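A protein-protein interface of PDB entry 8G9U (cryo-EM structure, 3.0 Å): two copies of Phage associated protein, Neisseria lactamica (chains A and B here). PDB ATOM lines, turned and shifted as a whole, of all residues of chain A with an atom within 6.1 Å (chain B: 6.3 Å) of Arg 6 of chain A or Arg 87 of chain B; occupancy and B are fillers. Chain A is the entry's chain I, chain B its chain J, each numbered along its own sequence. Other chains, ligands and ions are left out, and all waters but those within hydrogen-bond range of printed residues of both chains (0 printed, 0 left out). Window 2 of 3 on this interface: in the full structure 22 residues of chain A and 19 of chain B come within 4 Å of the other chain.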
ATOM      1  N   ASP A   3      14.363   7.328  14.840  1.00  0.00           N
ATOM      2  CA  ASP A   3      13.128   7.237  15.602  1.00  0.00           C
ATOM      3  C   ASP A   3      13.123   5.853  16.238  1.00  0.00           C
ATOM      4  O   ASP A   3      12.617   4.891  15.660  1.00  0.00           O
ATOM      5  CB  ASP A   3      11.912   7.466  14.712  1.00  0.00           C
ATOM      6  CG  ASP A   3      10.774   8.146  15.446  1.00  0.00           C
ATOM      7  OD1 ASP A   3      11.039   8.820  16.465  1.00  0.00           O
ATOM      8  OD2 ASP A   3       9.614   8.005  15.012  1.00  0.00           O
ATOM      9  N   ARG A   4      13.702   5.758  17.434  1.00  0.00           N
ATOM     10  CA  ARG A   4      13.867   4.464  18.076  1.00  0.00           C
ATOM     11  C   ARG A   4      12.539   3.804  18.388  1.00  0.00           C
ATOM     12  O   ARG A   4      12.503   2.597  18.654  1.00  0.00           O
ATOM     13  CB  ARG A   4      14.667   4.623  19.358  1.00  0.00           C
ATOM     14  CG  ARG A   4      16.067   5.115  19.138  1.00  0.00           C
ATOM     15  CD  ARG A   4      16.899   4.866  20.354  1.00  0.00           C
ATOM     16  NE  ARG A   4      16.840   3.473  20.768  1.00  0.00           N
ATOM     17  CZ  ARG A   4      17.537   2.505  20.191  1.00  0.00           C
ATOM     18  NH1 ARG A   4      17.442   1.258  20.625  1.00  0.00           N
ATOM     19  NH2 ARG A   4      18.340   2.788  19.182  1.00  0.00           N
ATOM     20  N   ASN A   5      11.453   4.564  18.374  1.00  0.00           N
ATOM     21  CA  ASN A   5      10.119   4.061  18.662  1.00  0.00           C
ATOM     22  C   ASN A   5       9.193   4.252  17.474  1.00  0.00           C
ATOM     23  O   ASN A   5       8.023   4.602  17.620  1.00  0.00           O
ATOM     24  CB  ASN A   5       9.567   4.723  19.916  1.00  0.00           C
ATOM     25  CG  ASN A   5      10.252   6.035  20.222  1.00  0.00           C
ATOM     26  OD1 ASN A   5      10.515   6.840  19.329  1.00  0.00           O
ATOM     27  ND2 ASN A   5      10.578   6.242  21.490  1.00  0.00           N
ATOM     28  N   ARG A   6       9.716   4.002  16.275  1.00  0.00           N
ATOM     29  CA  ARG A   6       8.969   4.300  15.064  1.00  0.00           C
ATOM     30  C   ARG A   6       7.851   3.296  14.837  1.00  0.00           C
ATOM     31  O   ARG A   6       6.773   3.659  14.357  1.00  0.00           O
ATOM     32  CB  ARG A   6       9.899   4.283  13.870  1.00  0.00           C
ATOM     33  CG  ARG A   6       9.220   4.617  12.578  1.00  0.00           C
ATOM     34  CD  ARG A   6       8.953   6.090  12.485  1.00  0.00           C
ATOM     35  NE  ARG A   6       8.356   6.409  11.199  1.00  0.00           N
ATOM     36  CZ  ARG A   6       9.058   6.708  10.113  1.00  0.00           C
ATOM     37  NH1 ARG A   6       8.433   6.977   8.978  1.00  0.00           N
ATOM     38  NH2 ARG A   6      10.381   6.725  10.155  1.00  0.00           N
ATOM     39  N   GLN A   7       8.117   2.022  15.127  1.00  0.00           N
ATOM     40  CA  GLN A   7       7.159   0.932  14.991  1.00  0.00           C
ATOM     41  C   GLN A   7       6.881   0.598  13.529  1.00  0.00           C
ATOM     42  O   GLN A   7       6.183  -0.378  13.243  1.00  0.00           O
ATOM     43  CB  GLN A   7       5.849   1.268  15.720  1.00  0.00           C
ATOM     44  CG  GLN A   7       5.930   1.298  17.249  1.00  0.00           C
ATOM     45  CD  GLN A   7       6.152  -0.063  17.876  1.00  0.00           C
ATOM     46  OE1 GLN A   7       6.458  -1.034  17.191  1.00  0.00           O
ATOM     47  NE2 GLN A   7       6.026  -0.131  19.195  1.00  0.00           N
ATOM     48  N   ASP A   8       7.428   1.377  12.594  1.00  0.00           N
ATOM     49  CA  ASP A   8       7.297   1.052  11.176  1.00  0.00           C
ATOM     50  C   ASP A   8       8.131  -0.178  10.879  1.00  0.00           C
ATOM     51  O   ASP A   8       9.362  -0.107  10.890  1.00  0.00           O
ATOM     52  CB  ASP A   8       7.742   2.215  10.296  1.00  0.00           C
ATOM     53  CG  ASP A   8       6.742   3.344  10.267  1.00  0.00           C
ATOM     54  OD1 ASP A   8       5.535   3.072  10.416  1.00  0.00           O
ATOM     55  OD2 ASP A   8       7.157   4.503  10.072  1.00  0.00           O
ATOM     56  N   TYR A  11      11.150   0.165   9.087  1.00  0.00           N
ATOM     57  CA  TYR A  11      12.165   0.944   9.784  1.00  0.00           C
ATOM     58  C   TYR A  11      12.780   0.150  10.923  1.00  0.00           C
ATOM     59  O   TYR A  11      13.996   0.188  11.126  1.00  0.00           O
ATOM     60  CB  TYR A  11      11.556   2.259  10.265  1.00  0.00           C
ATOM     61  CG  TYR A  11      12.523   3.298  10.781  1.00  0.00           C
ATOM     62  CD1 TYR A  11      13.856   3.207  10.556  1.00  0.00           C
ATOM     63  CD2 TYR A  11      12.069   4.440  11.379  1.00  0.00           C
ATOM     64  CE1 TYR A  11      14.723   4.173  11.012  1.00  0.00           C
ATOM     65  CE2 TYR A  11      12.912   5.409  11.827  1.00  0.00           C
ATOM     66  CZ  TYR A  11      14.242   5.273  11.637  1.00  0.00           C
ATOM     67  OH  TYR A  11      15.093   6.250  12.078  1.00  0.00           O
ATOM     68  N   VAL A  12      11.967  -0.589  11.674  1.00  0.00           N
ATOM     69  CA  VAL A  12      12.567  -1.378  12.741  1.00  0.00           C
ATOM     70  C   VAL A  12      13.411  -2.501  12.168  1.00  0.00           C
ATOM     71  O   VAL A  12      14.441  -2.847  12.741  1.00  0.00           O
ATOM     72  CB  VAL A  12      11.515  -1.905  13.730  1.00  0.00           C
ATOM     73  CG1 VAL A  12      10.247  -1.104  13.634  1.00  0.00           C
ATOM     74  CG2 VAL A  12      11.235  -3.367  13.493  1.00  0.00           C
ATOM     75  N   ARG A  15      16.672  -0.933  11.168  1.00  0.00           N
ATOM     76  CA  ARG A  15      17.475  -0.739  12.366  1.00  0.00           C
ATOM     77  C   ARG A  15      18.077  -2.051  12.825  1.00  0.00           C
ATOM     78  O   ARG A  15      19.248  -2.121  13.219  1.00  0.00           O
ATOM     79  CB  ARG A  15      16.613  -0.143  13.467  1.00  0.00           C
ATOM     80  CG  ARG A  15      16.137   1.239  13.177  1.00  0.00           C
ATOM     81  CD  ARG A  15      15.285   1.720  14.304  1.00  0.00           C
ATOM     82  NE  ARG A  15      16.028   1.683  15.550  1.00  0.00           N
ATOM     83  CZ  ARG A  15      15.564   1.140  16.663  1.00  0.00           C
ATOM     84  NH1 ARG A  15      14.355   0.609  16.679  1.00  0.00           N
ATOM     85  NH2 ARG A  15      16.301   1.136  17.758  1.00  0.00           N
ATOM     86  N   HIS A  84       9.757  -3.735  18.683  1.00  0.00           N
ATOM     87  CA  HIS A  84       8.937  -3.074  17.686  1.00  0.00           C
ATOM     88  C   HIS A  84       8.645  -3.967  16.504  1.00  0.00           C
ATOM     89  O   HIS A  84       7.953  -3.540  15.577  1.00  0.00           O
ATOM     90  CB  HIS A  84       9.631  -1.801  17.223  1.00  0.00           C
ATOM     91  CG  HIS A  84       9.999  -0.889  18.345  1.00  0.00           C
ATOM     92  ND1 HIS A  84       9.619   0.431  18.393  1.00  0.00           N
ATOM     93  CD2 HIS A  84      10.743  -1.106  19.454  1.00  0.00           C
ATOM     94  CE1 HIS A  84      10.089   0.981  19.497  1.00  0.00           C
ATOM     95  NE2 HIS A  84      10.782   0.072  20.154  1.00  0.00           N
ATOM     96  N   GLU A  95       6.514   1.243   1.014  1.00  0.00           N
ATOM     97  CA  GLU A  95       6.849   2.192   2.064  1.00  0.00           C
ATOM     98  C   GLU A  95       7.877   1.588   2.995  1.00  0.00           C
ATOM     99  O   GLU A  95       8.929   2.175   3.264  1.00  0.00           O
ATOM    100  CB  GLU A  95       5.589   2.554   2.844  1.00  0.00           C
ATOM    101  CG  GLU A  95       5.800   3.573   3.937  1.00  0.00           C
ATOM    102  CD  GLU A  95       5.324   4.957   3.565  1.00  0.00           C
ATOM    103  OE1 GLU A  95       4.535   5.082   2.610  1.00  0.00           O
ATOM    104  OE2 GLU A  95       5.740   5.917   4.243  1.00  0.00           O
ATOM    105  N   LEU A  99      11.743   2.342   4.002  1.00  0.00           N
ATOM    106  CA  LEU A  99      12.035   2.550   5.408  1.00  0.00           C
ATOM    107  C   LEU A  99      13.032   1.543   5.944  1.00  0.00           C
ATOM    108  O   LEU A  99      13.653   1.803   6.967  1.00  0.00           O
ATOM    109  CB  LEU A  99      10.762   2.507   6.237  1.00  0.00           C
ATOM    110  CG  LEU A  99      10.101   3.872   6.333  1.00  0.00           C
ATOM    111  CD1 LEU A  99       8.638   3.760   6.046  1.00  0.00           C
ATOM    112  CD2 LEU A  99      10.312   4.452   7.703  1.00  0.00           C
ATOM    113  N   ILE A 102      16.151   3.260   5.218  1.00  0.00           N
ATOM    114  CA  ILE A 102      16.144   4.322   6.216  1.00  0.00           C
ATOM    115  C   ILE A 102      16.628   3.786   7.549  1.00  0.00           C
ATOM    116  O   ILE A 102      17.464   4.394   8.211  1.00  0.00           O
ATOM    117  CB  ILE A 102      14.739   4.922   6.357  1.00  0.00           C
ATOM    118  CG1 ILE A 102      14.294   5.538   5.053  1.00  0.00           C
ATOM    119  CG2 ILE A 102      14.737   5.975   7.418  1.00  0.00           C
ATOM    120  CD1 ILE A 102      15.181   6.600   4.633  1.00  0.00           C
ATOM    121  N   HIS A 106      19.855   4.952   9.516  1.00  0.00           N
ATOM    122  CA  HIS A 106      19.582   5.622  10.778  1.00  0.00           C
ATOM    123  C   HIS A 106      20.251   4.903  11.934  1.00  0.00           C
ATOM    124  O   HIS A 106      20.985   5.512  12.715  1.00  0.00           O
ATOM    125  CB  HIS A 106      18.079   5.676  11.009  1.00  0.00           C
ATOM    126  CG  HIS A 106      17.394   6.779  10.278  1.00  0.00           C
ATOM    127  ND1 HIS A 106      16.519   7.644  10.893  1.00  0.00           N
ATOM    128  CD2 HIS A 106      17.474   7.177   8.991  1.00  0.00           C
ATOM    129  CE1 HIS A 106      16.070   8.513  10.007  1.00  0.00           C
ATOM    130  NE2 HIS A 106      16.635   8.253   8.845  1.00  0.00           N
ATOM    131  N   ILE B   9      12.600  16.855   2.200  1.00  0.00           N
ATOM    132  CA  ILE B   9      12.731  15.448   1.835  1.00  0.00           C
ATOM    133  C   ILE B   9      13.150  15.293   0.389  1.00  0.00           C
ATOM    134  O   ILE B   9      13.947  14.412   0.062  1.00  0.00           O
ATOM    135  CB  ILE B   9      11.436  14.675   2.133  1.00  0.00           C
ATOM    136  CG1 ILE B   9      11.712  13.186   2.012  1.00  0.00           C
ATOM    137  CG2 ILE B   9      10.316  15.084   1.201  1.00  0.00           C
ATOM    138  CD1 ILE B   9      12.689  12.688   3.023  1.00  0.00           C
ATOM    139  N   LEU B  13      16.649  13.547  -0.452  1.00  0.00           N
ATOM    140  CA  LEU B  13      16.682  12.401  -1.353  1.00  0.00           C
ATOM    141  C   LEU B  13      17.545  12.679  -2.561  1.00  0.00           C
ATOM    142  O   LEU B  13      18.181  11.772  -3.094  1.00  0.00           O
ATOM    143  CB  LEU B  13      15.288  12.016  -1.804  1.00  0.00           C
ATOM    144  CG  LEU B  13      14.471  11.441  -0.679  1.00  0.00           C
ATOM    145  CD1 LEU B  13      13.160  11.151  -1.254  1.00  0.00           C
ATOM    146  CD2 LEU B  13      15.128  10.202  -0.193  1.00  0.00           C
ATOM    147  N   ILE B  48      10.002   5.912  -3.346  1.00  0.00           N
ATOM    148  CA  ILE B  48       9.777   4.570  -2.828  1.00  0.00           C
ATOM    149  C   ILE B  48      10.076   3.527  -3.884  1.00  0.00           C
ATOM    150  O   ILE B  48      10.534   2.426  -3.559  1.00  0.00           O
ATOM    151  CB  ILE B  48       8.347   4.418  -2.301  1.00  0.00           C
ATOM    152  CG1 ILE B  48       7.358   4.678  -3.424  1.00  0.00           C
ATOM    153  CG2 ILE B  48       8.119   5.318  -1.133  1.00  0.00           C
ATOM    154  CD1 ILE B  48       6.004   4.202  -3.113  1.00  0.00           C
ATOM    155  N   HIS B  84      18.044  12.811   7.761  1.00  0.00           N
ATOM    156  CA  HIS B  84      17.065  13.802   7.360  1.00  0.00           C
ATOM    157  C   HIS B  84      15.920  13.194   6.586  1.00  0.00           C
ATOM    158  O   HIS B  84      15.006  13.919   6.182  1.00  0.00           O
ATOM    159  CB  HIS B  84      17.747  14.879   6.528  1.00  0.00           C
ATOM    160  CG  HIS B  84      18.925  15.492   7.208  1.00  0.00           C
ATOM    161  ND1 HIS B  84      19.060  16.848   7.395  1.00  0.00           N
ATOM    162  CD2 HIS B  84      20.042  14.929   7.722  1.00  0.00           C
ATOM    163  CE1 HIS B  84      20.196  17.090   8.022  1.00  0.00           C
ATOM    164  NE2 HIS B  84      20.816  15.943   8.224  1.00  0.00           N
ATOM    165  N   CYS B  85      15.955  11.893   6.361  1.00  0.00           N
ATOM    166  CA  CYS B  85      14.938  11.191   5.596  1.00  0.00           C
ATOM    167  C   CYS B  85      14.248  10.228   6.555  1.00  0.00           C
ATOM    168  O   CYS B  85      14.691   9.098   6.747  1.00  0.00           O
ATOM    169  CB  CYS B  85      15.555  10.468   4.419  1.00  0.00           C
ATOM    170  SG  CYS B  85      14.367   9.635   3.379  1.00  0.00           S
ATOM    171  N   GLN B  86      13.164  10.696   7.172  1.00  0.00           N
ATOM    172  CA  GLN B  86      12.388   9.836   8.054  1.00  0.00           C
ATOM    173  C   GLN B  86      11.651   8.753   7.288  1.00  0.00           C
ATOM    174  O   GLN B  86      11.225   7.762   7.892  1.00  0.00           O
ATOM    175  CB  GLN B  86      11.404  10.678   8.856  1.00  0.00           C
ATOM    176  CG  GLN B  86      12.074  11.573   9.875  1.00  0.00           C
ATOM    177  CD  GLN B  86      13.010  10.805  10.786  1.00  0.00           C
ATOM    178  OE1 GLN B  86      12.673   9.723  11.269  1.00  0.00           O
ATOM    179  NE2 GLN B  86      14.193  11.356  11.021  1.00  0.00           N
ATOM    180  N   ARG B  87      11.497   8.924   5.982  1.00  0.00           N
ATOM    181  CA  ARG B  87      10.812   7.975   5.121  1.00  0.00           C
ATOM    182  C   ARG B  87      11.072   8.373   3.684  1.00  0.00           C
ATOM    183  O   ARG B  87      11.175   9.561   3.379  1.00  0.00           O
ATOM    184  CB  ARG B  87       9.308   7.948   5.410  1.00  0.00           C
ATOM    185  CG  ARG B  87       8.631   9.301   5.261  1.00  0.00           C
ATOM    186  CD  ARG B  87       7.139   9.196   5.491  1.00  0.00           C
ATOM    187  NE  ARG B  87       6.506   8.324   4.512  1.00  0.00           N
ATOM    188  CZ  ARG B  87       6.141   8.728   3.301  1.00  0.00           C
ATOM    189  NH1 ARG B  87       5.578   7.879   2.455  1.00  0.00           N
ATOM    190  NH2 ARG B  87       6.308   9.995   2.951  1.00  0.00           N
ATOM    191  N   PHE B  88      11.197   7.387   2.817  1.00  0.00           N
ATOM    192  CA  PHE B  88      11.203   7.705   1.404  1.00  0.00           C
ATOM    193  C   PHE B  88       9.777   8.051   1.029  1.00  0.00           C
ATOM    194  O   PHE B  88       8.899   7.188   1.139  1.00  0.00           O
ATOM    195  CB  PHE B  88      11.712   6.535   0.583  1.00  0.00           C
ATOM    196  CG  PHE B  88      13.155   6.254   0.788  1.00  0.00           C
ATOM    197  CD1 PHE B  88      14.025   7.272   1.050  1.00  0.00           C
ATOM    198  CD2 PHE B  88      13.638   4.973   0.746  1.00  0.00           C
ATOM    199  CE1 PHE B  88      15.352   7.024   1.250  1.00  0.00           C
ATOM    200  CE2 PHE B  88      14.966   4.717   0.953  1.00  0.00           C
ATOM    201  CZ  PHE B  88      15.823   5.745   1.203  1.00  0.00           C
ATOM    202  N   PRO B  89       9.487   9.280   0.632  1.00  0.00           N
ATOM    203  CA  PRO B  89       8.109   9.645   0.333  1.00  0.00           C
ATOM    204  C   PRO B  89       7.585   8.862  -0.845  1.00  0.00           C
ATOM    205  O   PRO B  89       8.314   8.543  -1.783  1.00  0.00           O
ATOM    206  CB  PRO B  89       8.201  11.138   0.019  1.00  0.00           C
ATOM    207  CG  PRO B  89       9.577  11.323  -0.420  1.00  0.00           C
ATOM    208  CD  PRO B  89      10.398  10.396   0.399  1.00  0.00           C
ATOM    209  N   ASN B  90       6.296   8.546  -0.776  1.00  0.00           N
ATOM    210  CA  ASN B  90       5.663   7.782  -1.835  1.00  0.00           C
ATOM    211  C   ASN B  90       5.880   8.471  -3.172  1.00  0.00           C
ATOM    212  O   ASN B  90       6.570   7.948  -4.052  1.00  0.00           O
ATOM    213  CB  ASN B  90       4.178   7.624  -1.522  1.00  0.00           C
ATOM    214  CG  ASN B  90       3.888   6.411  -0.672  1.00  0.00           C
ATOM    215  OD1 ASN B  90       4.678   5.475  -0.611  1.00  0.00           O
ATOM    216  ND2 ASN B  90       2.755   6.432   0.014  1.00  0.00           N
ATOM    217  N   HIS B  91       5.347   9.676  -3.318  1.00  0.00           N
ATOM    218  CA  HIS B  91       5.596  10.520  -4.474  1.00  0.00           C
ATOM    219  C   HIS B  91       6.192  11.829  -3.997  1.00  0.00           C
ATOM    220  O   HIS B  91       5.629  12.476  -3.113  1.00  0.00           O
ATOM    221  CB  HIS B  91       4.309  10.793  -5.240  1.00  0.00           C
ATOM    222  CG  HIS B  91       4.521  11.398  -6.583  1.00  0.00           C
ATOM    223  ND1 HIS B  91       5.202  12.587  -6.766  1.00  0.00           N
ATOM    224  CD2 HIS B  91       4.117  11.014  -7.813  1.00  0.00           C
ATOM    225  CE1 HIS B  91       5.227  12.887  -8.046  1.00  0.00           C
ATOM    226  NE2 HIS B  91       4.571  11.948  -8.709  1.00  0.00           N
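Arg 6 of chain A touches Arg 87 of chain B (NH1 to CB, 3.8 Å).
Gln 86 of chain B touches Leu 99 of chain A.
Cys 85 of chain B touches Ile 102 of chain A.
Ile 102 of chain A touches Gln 86 of chain B (CG2 to O, 3.97 Å).
Phe 88 of chain B touches Ile 102 of chain A.
His 106 of chain A touches Gln 86 of chain B.
Arg 6 of chain A touches just these residues of chain B: Gln 86 and Arg 87.
Printed residues of chain B within 4 Å of Leu 99 of chain A: Gln 86 (3.4 Å).
Of the printed residues of chain B, His 106 of chain A touches Cys 85 (3.0 Å) and Gln 86 (3.6 Å).
Printed residues of chain A within 4 Å of Arg 87 of chain B: Arg 6 (3.8 Å) and Glu 95 (2.5 Å).
1 position is printed for both chains.
OD2 of Asp 8 of chain A is in salt-bridge range of NE of Arg 6 of chain A (2.5 Å).
O of Arg 87 of chain B sits at hydrogen-bond distance from SG of Cys 85 of chain B, at 3.2 Å.
Of the 14 printed residues of chain A, 5 touch a printed residue of chain B.
Hydrophobic or aromatic side chains of chain A that line the printed part of chain B: Leu 99, Ile 102 and His 106.
Hydrophobic or aromatic side chains of chain B that line the printed part of chain A: Phe 88.
The backbone carbonyl oxygen (O) of Gln 86 of chain B lies within hydrogen-bond range of the guanidinium group (NH2) of Arg 6 of chain A (2.6 Å).
OE2 of Glu 95 of chain A lies within salt-bridge range of NE of Arg 87 of chain B.
The side-chain amide oxygen (OD1) of Asn 90 of chain B lies close to the side-chain carboxylate (OE1) of Glu 95 of chain A (3.2 Å).
A ring nitrogen (NE2) of His 106 of chain A lies within hydrogen-bond range of the backbone carbonyl oxygen (O) of Cys 85 of chain B (3.0 Å).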
